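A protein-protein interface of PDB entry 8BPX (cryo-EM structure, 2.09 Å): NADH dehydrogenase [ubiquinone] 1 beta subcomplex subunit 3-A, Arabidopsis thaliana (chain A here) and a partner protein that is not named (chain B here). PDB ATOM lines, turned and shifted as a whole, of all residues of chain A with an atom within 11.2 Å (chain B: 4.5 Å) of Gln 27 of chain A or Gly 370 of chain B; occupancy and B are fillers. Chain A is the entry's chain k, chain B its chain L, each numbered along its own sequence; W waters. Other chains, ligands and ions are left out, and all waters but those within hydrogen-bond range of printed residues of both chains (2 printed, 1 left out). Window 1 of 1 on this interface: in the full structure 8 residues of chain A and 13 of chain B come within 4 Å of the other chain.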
ATOM      1  N   TRP A  18      30.037  12.287  11.920  1.00  0.00           N
ATOM      2  CA  TRP A  18      28.677  11.845  11.632  1.00  0.00           C
ATOM      3  C   TRP A  18      28.374  10.475  12.224  1.00  0.00           C
ATOM      4  O   TRP A  18      27.201  10.127  12.383  1.00  0.00           O
ATOM      5  CB  TRP A  18      28.443  11.829  10.120  1.00  0.00           C
ATOM      6  CG  TRP A  18      29.200  10.759   9.397  1.00  0.00           C
ATOM      7  CD1 TRP A  18      30.430  10.875   8.825  1.00  0.00           C
ATOM      8  CD2 TRP A  18      28.782   9.409   9.178  1.00  0.00           C
ATOM      9  NE1 TRP A  18      30.802   9.686   8.258  1.00  0.00           N
ATOM     10  CE2 TRP A  18      29.808   8.767   8.457  1.00  0.00           C
ATOM     11  CE3 TRP A  18      27.640   8.679   9.518  1.00  0.00           C
ATOM     12  CZ2 TRP A  18      29.728   7.436   8.071  1.00  0.00           C
ATOM     13  CZ3 TRP A  18      27.562   7.358   9.133  1.00  0.00           C
ATOM     14  CH2 TRP A  18      28.599   6.749   8.418  1.00  0.00           C
ATOM     15  N   ARG A  19      29.398   9.696  12.559  1.00  0.00           N
ATOM     16  CA  ARG A  19      29.190   8.382  13.149  1.00  0.00           C
ATOM     17  C   ARG A  19      28.660   8.454  14.574  1.00  0.00           C
ATOM     18  O   ARG A  19      28.284   7.419  15.130  1.00  0.00           O
ATOM     19  CB  ARG A  19      30.489   7.586  13.101  1.00  0.00           C
ATOM     20  CG  ARG A  19      30.749   6.971  11.740  1.00  0.00           C
ATOM     21  CD  ARG A  19      32.168   6.476  11.607  1.00  0.00           C
ATOM     22  NE  ARG A  19      32.655   6.633  10.245  1.00  0.00           N
ATOM     23  CZ  ARG A  19      32.580   5.695   9.313  1.00  0.00           C
ATOM     24  NH1 ARG A  19      32.009   4.526   9.555  1.00  0.00           N
ATOM     25  NH2 ARG A  19      33.078   5.939   8.106  1.00  0.00           N
ATOM     26  N   LYS A  20      28.624   9.641  15.175  1.00  0.00           N
ATOM     27  CA  LYS A  20      27.919   9.859  16.429  1.00  0.00           C
ATOM     28  C   LYS A  20      26.433  10.106  16.211  1.00  0.00           C
ATOM     29  O   LYS A  20      25.771  10.661  17.093  1.00  0.00           O
ATOM     30  CB  LYS A  20      28.539  11.029  17.195  1.00  0.00           C
ATOM     31  CG  LYS A  20      30.042  10.960  17.378  1.00  0.00           C
ATOM     32  CD  LYS A  20      30.511   9.559  17.730  1.00  0.00           C
ATOM     33  CE  LYS A  20      31.971   9.556  18.149  1.00  0.00           C
ATOM     34  NZ  LYS A  20      32.203   8.777  19.398  1.00  0.00           N
ATOM     35  N   HIS A  21      25.907   9.705  15.055  1.00  0.00           N
ATOM     36  CA  HIS A  21      24.484   9.825  14.773  1.00  0.00           C
ATOM     37  C   HIS A  21      23.681   9.154  15.884  1.00  0.00           C
ATOM     38  O   HIS A  21      24.042   8.058  16.329  1.00  0.00           O
ATOM     39  CB  HIS A  21      24.156   9.169  13.428  1.00  0.00           C
ATOM     40  CG  HIS A  21      23.015   9.805  12.698  1.00  0.00           C
ATOM     41  ND1 HIS A  21      21.705   9.677  13.109  1.00  0.00           N
ATOM     42  CD2 HIS A  21      22.980  10.533  11.558  1.00  0.00           C
ATOM     43  CE1 HIS A  21      20.916  10.325  12.271  1.00  0.00           C
ATOM     44  NE2 HIS A  21      21.666  10.854  11.319  1.00  0.00           N
ATOM     45  N   PRO A  22      22.601   9.782  16.357  1.00  0.00           N
ATOM     46  CA  PRO A  22      21.877   9.222  17.512  1.00  0.00           C
ATOM     47  C   PRO A  22      21.387   7.799  17.303  1.00  0.00           C
ATOM     48  O   PRO A  22      21.547   6.964  18.200  1.00  0.00           O
ATOM     49  CB  PRO A  22      20.708  10.197  17.687  1.00  0.00           C
ATOM     50  CG  PRO A  22      21.197  11.474  17.109  1.00  0.00           C
ATOM     51  CD  PRO A  22      22.088  11.106  15.968  1.00  0.00           C
ATOM     52  N   MET A  23      20.830   7.481  16.135  1.00  0.00           N
ATOM     53  CA  MET A  23      20.274   6.157  15.903  1.00  0.00           C
ATOM     54  C   MET A  23      21.198   5.264  15.087  1.00  0.00           C
ATOM     55  O   MET A  23      20.767   4.219  14.592  1.00  0.00           O
ATOM     56  CB  MET A  23      18.890   6.256  15.260  1.00  0.00           C
ATOM     57  CG  MET A  23      18.757   7.119  14.030  1.00  0.00           C
ATOM     58  SD  MET A  23      16.988   7.259  13.688  1.00  0.00           S
ATOM     59  CE  MET A  23      16.915   7.090  11.911  1.00  0.00           C
ATOM     60  N   LEU A  24      22.462   5.654  14.949  1.00  0.00           N
ATOM     61  CA  LEU A  24      23.508   4.771  14.462  1.00  0.00           C
ATOM     62  C   LEU A  24      24.409   4.272  15.580  1.00  0.00           C
ATOM     63  O   LEU A  24      25.238   3.388  15.341  1.00  0.00           O
ATOM     64  CB  LEU A  24      24.361   5.491  13.408  1.00  0.00           C
ATOM     65  CG  LEU A  24      23.731   5.710  12.034  1.00  0.00           C
ATOM     66  CD1 LEU A  24      24.805   5.831  10.971  1.00  0.00           C
ATOM     67  CD2 LEU A  24      22.750   4.595  11.695  1.00  0.00           C
ATOM     68  N   SER A  25      24.265   4.811  16.783  1.00  0.00           N
ATOM     69  CA  SER A  25      25.155   4.540  17.900  1.00  0.00           C
ATOM     70  C   SER A  25      24.389   3.921  19.059  1.00  0.00           C
ATOM     71  O   SER A  25      23.157   3.956  19.114  1.00  0.00           O
ATOM     72  CB  SER A  25      25.845   5.827  18.357  1.00  0.00           C
ATOM     73  OG  SER A  25      24.889   6.842  18.600  1.00  0.00           O
ATOM     74  N   ASN A  26      25.153   3.368  20.005  1.00  0.00           N
ATOM     75  CA  ASN A  26      24.605   2.736  21.205  1.00  0.00           C
ATOM     76  C   ASN A  26      23.611   1.636  20.840  1.00  0.00           C
ATOM     77  O   ASN A  26      22.558   1.480  21.459  1.00  0.00           O
ATOM     78  CB  ASN A  26      23.966   3.775  22.129  1.00  0.00           C
ATOM     79  CG  ASN A  26      24.993   4.667  22.802  1.00  0.00           C
ATOM     80  OD1 ASN A  26      26.159   4.295  22.940  1.00  0.00           O
ATOM     81  ND2 ASN A  26      24.563   5.848  23.227  1.00  0.00           N
ATOM     82  N   GLN A  27      23.964   0.859  19.817  1.00  0.00           N
ATOM     83  CA  GLN A  27      23.086  -0.190  19.321  1.00  0.00           C
ATOM     84  C   GLN A  27      23.077  -1.431  20.205  1.00  0.00           C
ATOM     85  O   GLN A  27      22.229  -2.304  20.000  1.00  0.00           O
ATOM     86  CB  GLN A  27      23.482  -0.568  17.893  1.00  0.00           C
ATOM     87  CG  GLN A  27      23.289   0.558  16.902  1.00  0.00           C
ATOM     88  CD  GLN A  27      21.840   0.968  16.792  1.00  0.00           C
ATOM     89  OE1 GLN A  27      20.960   0.125  16.643  1.00  0.00           O
ATOM     90  NE2 GLN A  27      21.581   2.263  16.884  1.00  0.00           N
ATOM     91  N   MET A  28      23.979  -1.527  21.182  1.00  0.00           N
ATOM     92  CA  MET A  28      23.961  -2.672  22.086  1.00  0.00           C
ATOM     93  C   MET A  28      22.721  -2.669  22.966  1.00  0.00           C
ATOM     94  O   MET A  28      22.317  -3.721  23.472  1.00  0.00           O
ATOM     95  CB  MET A  28      25.222  -2.687  22.943  1.00  0.00           C
ATOM     96  CG  MET A  28      26.410  -3.346  22.264  1.00  0.00           C
ATOM     97  SD  MET A  28      26.135  -5.088  21.890  1.00  0.00           S
ATOM     98  CE  MET A  28      26.396  -5.820  23.500  1.00  0.00           C
ATOM     99  N   ARG A  29      22.093  -1.507  23.146  1.00  0.00           N
ATOM    100  CA  ARG A  29      20.828  -1.454  23.860  1.00  0.00           C
ATOM    101  C   ARG A  29      19.668  -2.011  23.044  1.00  0.00           C
ATOM    102  O   ARG A  29      18.599  -2.258  23.612  1.00  0.00           O
ATOM    103  CB  ARG A  29      20.536  -0.016  24.294  1.00  0.00           C
ATOM    104  CG  ARG A  29      21.477   0.542  25.337  1.00  0.00           C
ATOM    105  CD  ARG A  29      21.081   1.951  25.739  1.00  0.00           C
ATOM    106  NE  ARG A  29      22.023   2.527  26.693  1.00  0.00           N
ATOM    107  CZ  ARG A  29      21.990   3.779  27.129  1.00  0.00           C
ATOM    108  NH1 ARG A  29      21.076   4.637  26.701  1.00  0.00           N
ATOM    109  NH2 ARG A  29      22.897   4.183  28.013  1.00  0.00           N
ATOM    110  N   HIS A  30      19.837  -2.225  21.747  1.00  0.00           N
ATOM    111  CA  HIS A  30      18.795  -2.775  20.850  1.00  0.00           C
ATOM    112  C   HIS A  30      19.022  -4.239  20.545  1.00  0.00           C
ATOM    113  O   HIS A  30      18.321  -4.749  19.700  1.00  0.00           O
ATOM    114  CB  HIS A  30      18.858  -1.998  19.545  1.00  0.00           C
ATOM    115  CG  HIS A  30      18.110  -0.717  19.607  1.00  0.00           C
ATOM    116  ND1 HIS A  30      18.658   0.429  20.132  1.00  0.00           N
ATOM    117  CD2 HIS A  30      16.845  -0.417  19.258  1.00  0.00           C
ATOM    118  CE1 HIS A  30      17.775   1.393  20.072  1.00  0.00           C
ATOM    119  NE2 HIS A  30      16.657   0.905  19.537  1.00  0.00           N
ATOM    120  N   ALA A  31      19.975  -4.870  21.190  1.00  0.00           N
ATOM    121  CA  ALA A  31      20.416  -6.230  20.866  1.00  0.00           C
ATOM    122  C   ALA A  31      19.409  -7.340  21.234  1.00  0.00           C
ATOM    123  O   ALA A  31      19.500  -8.366  20.664  1.00  0.00           O
ATOM    124  CB  ALA A  31      21.718  -6.376  21.565  1.00  0.00           C
ATOM    125  N   LEU A  32      18.546  -7.117  22.237  1.00  0.00           N
ATOM    126  CA  LEU A  32      17.594  -8.130  22.716  1.00  0.00           C
ATOM    127  C   LEU A  32      16.190  -7.542  22.630  1.00  0.00           C
ATOM    128  O   LEU A  32      15.601  -7.285  23.651  1.00  0.00           O
ATOM    129  CB  LEU A  32      18.061  -8.552  24.121  1.00  0.00           C
ATOM    130  CG  LEU A  32      19.446  -9.167  24.251  1.00  0.00           C
ATOM    131  CD1 LEU A  32      19.803  -9.302  25.721  1.00  0.00           C
ATOM    132  CD2 LEU A  32      19.526 -10.504  23.538  1.00  0.00           C
ATOM    133  N   PRO A  33      15.627  -7.351  21.419  1.00  0.00           N
ATOM    134  CA  PRO A  33      14.341  -6.725  21.224  1.00  0.00           C
ATOM    135  C   PRO A  33      13.228  -7.634  21.727  1.00  0.00           C
ATOM    136  O   PRO A  33      13.337  -8.801  21.603  1.00  0.00           O
ATOM    137  CB  PRO A  33      14.172  -6.572  19.693  1.00  0.00           C
ATOM    138  CG  PRO A  33      15.138  -7.549  19.076  1.00  0.00           C
ATOM    139  CD  PRO A  33      16.191  -7.799  20.128  1.00  0.00           C
ATOM    140  N   GLY B 369      27.714  -2.320  10.521  1.00  0.00           N
ATOM    141  CA  GLY B 369      27.690  -2.008  11.935  1.00  0.00           C
ATOM    142  C   GLY B 369      26.716  -0.895  12.255  1.00  0.00           C
ATOM    143  O   GLY B 369      26.411  -0.039  11.421  1.00  0.00           O
ATOM    144  N   GLY B 370      26.216  -0.908  13.486  1.00  0.00           N
ATOM    145  CA  GLY B 370      25.213   0.063  13.895  1.00  0.00           C
ATOM    146  C   GLY B 370      23.952  -0.010  13.066  1.00  0.00           C
ATOM    147  O   GLY B 370      23.346   1.024  12.763  1.00  0.00           O
ATOM    148  N   LEU B 371      23.539  -1.215  12.691  1.00  0.00           N
ATOM    149  CA  LEU B 371      22.428  -1.419  11.777  1.00  0.00           C
ATOM    150  C   LEU B 371      21.197  -2.007  12.454  1.00  0.00           C
ATOM    151  O   LEU B 371      20.170  -2.182  11.793  1.00  0.00           O
ATOM    152  CB  LEU B 371      22.879  -2.327  10.626  1.00  0.00           C
ATOM    153  CG  LEU B 371      23.192  -1.692   9.273  1.00  0.00           C
ATOM    154  CD1 LEU B 371      24.039  -0.441   9.413  1.00  0.00           C
ATOM    155  CD2 LEU B 371      23.889  -2.705   8.370  1.00  0.00           C
ATOM    156  N   ALA B 372      21.270  -2.312  13.752  1.00  0.00           N
ATOM    157  CA  ALA B 372      20.142  -2.944  14.434  1.00  0.00           C
ATOM    158  C   ALA B 372      18.901  -2.059  14.404  1.00  0.00           C
ATOM    159  O   ALA B 372      17.791  -2.543  14.159  1.00  0.00           O
ATOM    160  CB  ALA B 372      20.527  -3.282  15.874  1.00  0.00           C
ATOM    161  N   SER B 373      19.068  -0.759  14.646  1.00  0.00           N
ATOM    162  CA  SER B 373      17.925   0.148  14.678  1.00  0.00           C
ATOM    163  C   SER B 373      17.402   0.482  13.288  1.00  0.00           C
ATOM    164  O   SER B 373      16.208   0.757  13.134  1.00  0.00           O
ATOM    165  CB  SER B 373      18.297   1.430  15.419  1.00  0.00           C
ATOM    166  OG  SER B 373      18.636   1.138  16.759  1.00  0.00           O
ATOM    167  N   THR B 441      27.896  -6.912  12.187  1.00  0.00           N
ATOM    168  CA  THR B 441      26.889  -6.411  11.264  1.00  0.00           C
ATOM    169  C   THR B 441      25.955  -5.396  11.916  1.00  0.00           C
ATOM    170  O   THR B 441      25.586  -4.404  11.280  1.00  0.00           O
ATOM    171  CB  THR B 441      26.090  -7.580  10.688  1.00  0.00           C
ATOM    172  OG1 THR B 441      26.990  -8.598  10.239  1.00  0.00           O
ATOM    173  CG2 THR B 441      25.217  -7.128   9.542  1.00  0.00           C
ATOM    174  N   PHE B 442      25.554  -5.609  13.167  1.00  0.00           N
ATOM    175  CA  PHE B 442      24.444  -4.831  13.699  1.00  0.00           C
ATOM    176  C   PHE B 442      24.758  -4.013  14.942  1.00  0.00           C
ATOM    177  O   PHE B 442      24.093  -3.001  15.166  1.00  0.00           O
ATOM    178  CB  PHE B 442      23.255  -5.751  14.014  1.00  0.00           C
ATOM    179  CG  PHE B 442      22.675  -6.425  12.809  1.00  0.00           C
ATOM    180  CD1 PHE B 442      21.798  -5.751  11.976  1.00  0.00           C
ATOM    181  CD2 PHE B 442      22.997  -7.737  12.507  1.00  0.00           C
ATOM    182  CE1 PHE B 442      21.257  -6.374  10.873  1.00  0.00           C
ATOM    183  CE2 PHE B 442      22.455  -8.358  11.402  1.00  0.00           C
ATOM    184  CZ  PHE B 442      21.588  -7.675  10.586  1.00  0.00           C
ATOM    185  N   LEU B 443      25.734  -4.407  15.753  1.00  0.00           N
ATOM    186  CA  LEU B 443      25.845  -3.860  17.100  1.00  0.00           C
ATOM    187  C   LEU B 443      27.047  -2.957  17.337  1.00  0.00           C
ATOM    188  O   LEU B 443      26.964  -2.078  18.194  1.00  0.00           O
ATOM    189  CB  LEU B 443      25.863  -4.999  18.128  1.00  0.00           C
ATOM    190  CG  LEU B 443      24.665  -5.935  17.976  1.00  0.00           C
ATOM    191  CD1 LEU B 443      24.641  -7.010  19.043  1.00  0.00           C
ATOM    192  CD2 LEU B 443      23.379  -5.127  18.006  1.00  0.00           C
ATOM    193  N   VAL B 444      28.150  -3.133  16.616  1.00  0.00           N
ATOM    194  CA  VAL B 444      29.335  -2.306  16.839  1.00  0.00           C
ATOM    195  C   VAL B 444      29.059  -0.897  16.329  1.00  0.00           C
ATOM    196  O   VAL B 444      28.153  -0.710  15.507  1.00  0.00           O
ATOM    197  CB  VAL B 444      30.584  -2.905  16.167  1.00  0.00           C
ATOM    198  CG1 VAL B 444      31.016  -4.181  16.879  1.00  0.00           C
ATOM    199  CG2 VAL B 444      30.350  -3.148  14.677  1.00  0.00           C
ATOM    200  N   THR B 446      29.199   2.064  13.889  1.00  0.00           N
ATOM    201  CA  THR B 446      29.155   1.792  12.458  1.00  0.00           C
ATOM    202  C   THR B 446      30.503   2.047  11.788  1.00  0.00           C
ATOM    203  O   THR B 446      31.181   3.044  12.055  1.00  0.00           O
ATOM    204  CB  THR B 446      28.062   2.630  11.784  1.00  0.00           C
ATOM    205  OG1 THR B 446      27.999   2.305  10.390  1.00  0.00           O
ATOM    206  CG2 THR B 446      28.326   4.118  11.935  1.00  0.00           C
HETATM  207  O   HOH W   1      27.964   4.791  15.032  1.00  0.00           O
HETATM  208  O   HOH W   2      16.859  -4.017  17.052  1.00  0.00           O
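Water W1 lies within hydrogen-bond range of O of Arg 19 of chain A, O of Leu 24 of chain A and N of Thr 446 of chain B.
Water W2 lies within hydrogen-bond range of the backbone carbonyl oxygen of His 30 of chain A (3.1 Å) and the backbone carbonyl oxygen of Ala 372 of chain B (3.4 Å).
Met 23 of chain A touches Ser 373 of chain B (O to CB, 3.8 Å).
CA of Gly 370 of chain B touches O of Leu 24 of chain A, at 3.6 Å.
Gln 27 of chain A touches Gly 370 of chain B.
Gln 27 of chain A touches Ala 372 of chain B (OE1 to CB, 3.5 Å).
Phe 442 of chain B touches Gln 27 of chain A.
O of Gln 27 of chain A touches CD2 of Leu 443 of chain B, at 3.6 Å.
Leu 443 of chain B touches Met 28 of chain A (CD1 to SD, 3.7 Å).
CB of Ala 31 of chain A touches CD1 of Leu 443 of chain B, 3.9 Å away.
OG of Ser 373 of chain B lies within hydrogen-bond range of OE1 of Gln 27 of chain A (2.5 Å).
The side-chain hydroxyl of Ser 373 of chain B sits at hydrogen-bond distance from a ring nitrogen (NE2) of His 30 of chain A (3.4 Å).
The backbone carbonyl oxygen (O) of Thr 446 of chain B is in hydrogen-bond range of the guanidinium group (NH1) of Arg 19 of chain A, at 3.0 Å.
Printed residues of chain A that touch a printed residue of chain B: Arg 19, Met 23, Leu 24, Gln 27, Met 28, His 30 and Ala 31.
Hydrophobic or aromatic side chains of chain A that line the printed part of chain B: Leu 24, Met 28, His 30 and Ala 31.
Of the 10 printed residues of chain B, 6 touch a printed residue of chain A.
Printed residues of chain B that touch a printed residue of chain A: Gly 370, Ala 372, Ser 373, Phe 442, Leu 443 and Thr 446.
Hydrophobic or aromatic side chains of chain B that line the printed part of chain A: Ala 372 and Leu 443.
Along chain B the printed residues that touch a printed residue of chain A span positions 370 to 446.
Among the printed residues, 11 pairs touch across the chains.
Among the printed residues, no Asp or Glu carboxylate lies within 4 Å of a Lys or Arg side-chain nitrogen of the other chain.
O of Gly 369 of chain B sits at hydrogen-bond distance from OG1 of Thr 446 of chain B, at 3.0 Å.
The backbone carbonyl oxygen of Phe 442 of chain B lies within hydrogen-bond range of the backbone NH of Gly 370 of chain B.
N of Leu 371 of chain B sits at hydrogen-bond distance from O of Phe 442 of chain B (3.1 Å).
The backbone NH (N) of Ala 372 of chain B is in hydrogen-bond range of the backbone carbonyl oxygen (O) of Phe 442 of chain B (3.2 Å).
O of Met 23 of chain A sits at hydrogen-bond distance from NE2 of Gln 27 of chain A (3.1 Å).
The backbone carbonyl oxygen (O) of Ser 25 of chain A is in hydrogen-bond range of the side-chain amide nitrogen (NE2) of Gln 27 of chain A, at 3.2 Å.
Of the printed residues of chain A, Gly 370 of chain B touches Leu 24 (3.6 Å) and Gln 27 (3.6 Å).
No residue of chain A comes within 4 Å of Gly 369 of chain B.
Leu 443 of chain B touches just these residues of chain A: Gln 27 (3.6 Å), Met 28 (3.7 Å) and Ala 31 (3.9 Å).
No residue of chain A comes within 4 Å of Val 444 of chain B.
Of the printed residues of chain A, Thr 446 of chain B touches Arg 19 (3.0 Å).
Of the printed residues of chain B, His 30 of chain A touches Ser 373 (3.4 Å).
Of the printed residues of chain B, Arg 19 of chain A touches Thr 446.
Printed residues of chain A within 4 Å of Phe 442 of chain B: Gln 27 (3.7 Å).
Arg 29 of chain A touches none of the printed residues of chain B.
The nearest printed residue of chain B that does not touch Gln 27 of chain A is Leu 371 of chain B (4.6 Å).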
